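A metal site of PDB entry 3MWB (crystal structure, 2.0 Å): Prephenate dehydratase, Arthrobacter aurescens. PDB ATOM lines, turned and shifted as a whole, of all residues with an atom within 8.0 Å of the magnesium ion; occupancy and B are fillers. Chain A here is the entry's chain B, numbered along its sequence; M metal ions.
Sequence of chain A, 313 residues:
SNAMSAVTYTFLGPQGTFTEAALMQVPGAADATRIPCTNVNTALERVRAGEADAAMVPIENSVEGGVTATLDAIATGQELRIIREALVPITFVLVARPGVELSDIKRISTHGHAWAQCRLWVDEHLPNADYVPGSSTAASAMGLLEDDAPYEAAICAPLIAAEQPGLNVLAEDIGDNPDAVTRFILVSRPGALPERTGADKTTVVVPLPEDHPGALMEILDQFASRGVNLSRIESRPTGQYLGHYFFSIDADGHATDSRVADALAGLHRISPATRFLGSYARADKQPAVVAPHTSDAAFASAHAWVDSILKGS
Residues that only touch the magnesium ion: Pro 165.
Of the 15 residues printed, 4 come within 4 Å of the magnesium ion.
The nearest printed residue that does not touch the magnesium ion is Ala 162 (4.4 Å).
The magnesium ion is bound by O of Ala 161 (2.2 Å).
O of Leu 167 is bound to the magnesium ion (2.3 Å).
The backbone carbonyl oxygen (O) of Gln 164 is bound to the magnesium ion, 2.3 Å away.
The magnesium ion has three donor atoms within binding distance.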
ATOM      1  N   VAL A  95      11.560  18.050  -9.662  1.00  0.00           N
ATOM      2  CA  VAL A  95      11.543  18.753  -8.373  1.00  0.00           C
ATOM      3  C   VAL A  95      10.196  18.652  -7.669  1.00  0.00           C
ATOM      4  O   VAL A  95       9.174  18.508  -8.318  1.00  0.00           O
ATOM      5  CB  VAL A  95      11.970  20.255  -8.518  1.00  0.00           C
ATOM      6  CG1 VAL A  95      13.374  20.373  -9.097  1.00  0.00           C
ATOM      7  CG2 VAL A  95      10.988  21.056  -9.401  1.00  0.00           C
ATOM      8  N   ALA A  96      10.235  18.700  -6.337  1.00  0.00           N
ATOM      9  CA  ALA A  96       9.031  18.783  -5.519  1.00  0.00           C
ATOM     10  C   ALA A  96       9.348  19.592  -4.262  1.00  0.00           C
ATOM     11  O   ALA A  96      10.527  19.905  -3.992  1.00  0.00           O
ATOM     12  CB  ALA A  96       8.539  17.380  -5.119  1.00  0.00           C
ATOM     13  N   PRO A  98       9.748  20.111  -0.177  1.00  0.00           N
ATOM     14  CA  PRO A  98      10.356  19.214   0.813  1.00  0.00           C
ATOM     15  C   PRO A  98       9.329  18.288   1.456  1.00  0.00           C
ATOM     16  O   PRO A  98       8.191  18.700   1.654  1.00  0.00           O
ATOM     17  CB  PRO A  98      10.918  20.176   1.840  1.00  0.00           C
ATOM     18  CG  PRO A  98      11.326  21.357   1.017  1.00  0.00           C
ATOM     19  CD  PRO A  98      10.175  21.515   0.023  1.00  0.00           C
ATOM     20  N   PRO A 158      17.984  22.558 -14.214  1.00  0.00           N
ATOM     21  CA  PRO A 158      18.758  22.609 -12.963  1.00  0.00           C
ATOM     22  C   PRO A 158      18.876  24.032 -12.370  1.00  0.00           C
ATOM     23  O   PRO A 158      18.983  24.169 -11.152  1.00  0.00           O
ATOM     24  CB  PRO A 158      20.136  22.062 -13.381  1.00  0.00           C
ATOM     25  CG  PRO A 158      19.837  21.174 -14.560  1.00  0.00           C
ATOM     26  CD  PRO A 158      18.738  21.920 -15.302  1.00  0.00           C
ATOM     27  N   LEU A 159      18.829  25.066 -13.212  1.00  0.00           N
ATOM     28  CA  LEU A 159      18.914  26.461 -12.753  1.00  0.00           C
ATOM     29  C   LEU A 159      17.870  26.809 -11.693  1.00  0.00           C
ATOM     30  O   LEU A 159      18.206  27.270 -10.596  1.00  0.00           O
ATOM     31  CB  LEU A 159      18.814  27.454 -13.925  1.00  0.00           C
ATOM     32  CG  LEU A 159      18.737  28.965 -13.582  1.00  0.00           C
ATOM     33  CD1 LEU A 159      19.994  29.476 -12.843  1.00  0.00           C
ATOM     34  CD2 LEU A 159      18.471  29.817 -14.827  1.00  0.00           C
ATOM     35  N   ILE A 160      16.610  26.536 -12.029  1.00  0.00           N
ATOM     36  CA  ILE A 160      15.469  26.825 -11.187  1.00  0.00           C
ATOM     37  C   ILE A 160      15.559  26.031  -9.884  1.00  0.00           C
ATOM     38  O   ILE A 160      15.257  26.558  -8.803  1.00  0.00           O
ATOM     39  CB  ILE A 160      14.127  26.583 -12.011  1.00  0.00           C
ATOM     40  CG1 ILE A 160      13.171  27.787 -11.943  1.00  0.00           C
ATOM     41  CG2 ILE A 160      13.456  25.270 -11.662  1.00  0.00           C
ATOM     42  CD1 ILE A 160      13.185  28.518 -10.647  1.00  0.00           C
ATOM     43  N   ALA A 161      16.028  24.788  -9.975  1.00  0.00           N
ATOM     44  CA  ALA A 161      16.170  23.933  -8.800  1.00  0.00           C
ATOM     45  C   ALA A 161      17.185  24.474  -7.781  1.00  0.00           C
ATOM     46  O   ALA A 161      16.949  24.396  -6.573  1.00  0.00           O
ATOM     47  CB  ALA A 161      16.534  22.520  -9.220  1.00  0.00           C
ATOM     48  N   ALA A 162      18.284  25.037  -8.274  1.00  0.00           N
ATOM     49  CA  ALA A 162      19.352  25.585  -7.437  1.00  0.00           C
ATOM     50  C   ALA A 162      19.072  27.010  -6.941  1.00  0.00           C
ATOM     51  O   ALA A 162      19.542  27.393  -5.859  1.00  0.00           O
ATOM     52  CB  ALA A 162      20.701  25.542  -8.175  1.00  0.00           C
ATOM     53  N   GLU A 163      18.314  27.787  -7.723  1.00  0.00           N
ATOM     54  CA  GLU A 163      17.821  29.109  -7.310  1.00  0.00           C
ATOM     55  C   GLU A 163      16.787  29.046  -6.186  1.00  0.00           C
ATOM     56  O   GLU A 163      16.723  29.951  -5.376  1.00  0.00           O
ATOM     57  CB  GLU A 163      17.142  29.827  -8.476  1.00  0.00           C
ATOM     58  CG  GLU A 163      18.025  30.580  -9.435  1.00  0.00           C
ATOM     59  CD  GLU A 163      17.184  31.270 -10.510  1.00  0.00           C
ATOM     60  OE1 GLU A 163      17.737  32.100 -11.260  1.00  0.00           O
ATOM     61  OE2 GLU A 163      15.952  30.977 -10.588  1.00  0.00           O
ATOM     62  N   GLN A 164      15.954  28.000  -6.174  1.00  0.00           N
ATOM     63  CA  GLN A 164      14.812  27.960  -5.244  1.00  0.00           C
ATOM     64  C   GLN A 164      15.044  26.983  -4.086  1.00  0.00           C
ATOM     65  O   GLN A 164      14.968  25.760  -4.281  1.00  0.00           O
ATOM     66  CB  GLN A 164      13.516  27.631  -5.978  1.00  0.00           C
ATOM     67  CG  GLN A 164      13.155  28.632  -7.105  1.00  0.00           C
ATOM     68  CD  GLN A 164      12.829  30.029  -6.609  1.00  0.00           C
ATOM     69  OE1 GLN A 164      13.210  31.034  -7.241  1.00  0.00           O
ATOM     70  NE2 GLN A 164      12.110  30.119  -5.500  1.00  0.00           N
ATOM     71  N   PRO A 165      15.304  27.525  -2.868  1.00  0.00           N
ATOM     72  CA  PRO A 165      15.537  26.700  -1.691  1.00  0.00           C
ATOM     73  C   PRO A 165      14.296  25.872  -1.319  1.00  0.00           C
ATOM     74  O   PRO A 165      14.410  24.871  -0.610  1.00  0.00           O
ATOM     75  CB  PRO A 165      15.816  27.720  -0.592  1.00  0.00           C
ATOM     76  CG  PRO A 165      14.994  28.923  -1.035  1.00  0.00           C
ATOM     77  CD  PRO A 165      15.282  28.962  -2.518  1.00  0.00           C
ATOM     78  N   GLY A 166      13.135  26.287  -1.795  1.00  0.00           N
ATOM     79  CA  GLY A 166      11.880  25.583  -1.522  1.00  0.00           C
ATOM     80  C   GLY A 166      11.597  24.494  -2.519  1.00  0.00           C
ATOM     81  O   GLY A 166      10.561  23.838  -2.445  1.00  0.00           O
ATOM     82  N   LEU A 167      12.509  24.284  -3.479  1.00  0.00           N
ATOM     83  CA  LEU A 167      12.382  23.159  -4.390  1.00  0.00           C
ATOM     84  C   LEU A 167      13.494  22.121  -4.192  1.00  0.00           C
ATOM     85  O   LEU A 167      14.678  22.463  -4.199  1.00  0.00           O
ATOM     86  CB  LEU A 167      12.315  23.630  -5.853  1.00  0.00           C
ATOM     87  CG  LEU A 167      11.120  24.525  -6.236  1.00  0.00           C
ATOM     88  CD1 LEU A 167      11.216  24.954  -7.676  1.00  0.00           C
ATOM     89  CD2 LEU A 167       9.759  23.863  -5.946  1.00  0.00           C
ATOM     90  N   ASN A 168      13.092  20.861  -4.007  1.00  0.00           N
ATOM     91  CA  ASN A 168      14.004  19.746  -3.844  1.00  0.00           C
ATOM     92  C   ASN A 168      14.081  18.887  -5.120  1.00  0.00           C
ATOM     93  O   ASN A 168      13.068  18.550  -5.697  1.00  0.00           O
ATOM     94  CB  ASN A 168      13.566  18.847  -2.659  1.00  0.00           C
ATOM     95  CG  ASN A 168      13.866  19.469  -1.283  1.00  0.00           C
ATOM     96  OD1 ASN A 168      14.169  20.673  -1.138  1.00  0.00           O
ATOM     97  ND2 ASN A 168      13.775  18.611  -0.245  1.00  0.00           N
ATOM     98  N   VAL A 169      15.288  18.540  -5.547  1.00  0.00           N
ATOM     99  CA  VAL A 169      15.482  17.591  -6.653  1.00  0.00           C
ATOM    100  C   VAL A 169      15.195  16.182  -6.144  1.00  0.00           C
ATOM    101  O   VAL A 169      15.794  15.736  -5.154  1.00  0.00           O
ATOM    102  CB  VAL A 169      16.928  17.669  -7.190  1.00  0.00           C
ATOM    103  CG1 VAL A 169      17.237  16.528  -8.170  1.00  0.00           C
ATOM    104  CG2 VAL A 169      17.202  19.037  -7.810  1.00  0.00           C
HETATM  105 MG    MG M   1      16.411  23.953  -4.442  1.00  0.00          MG
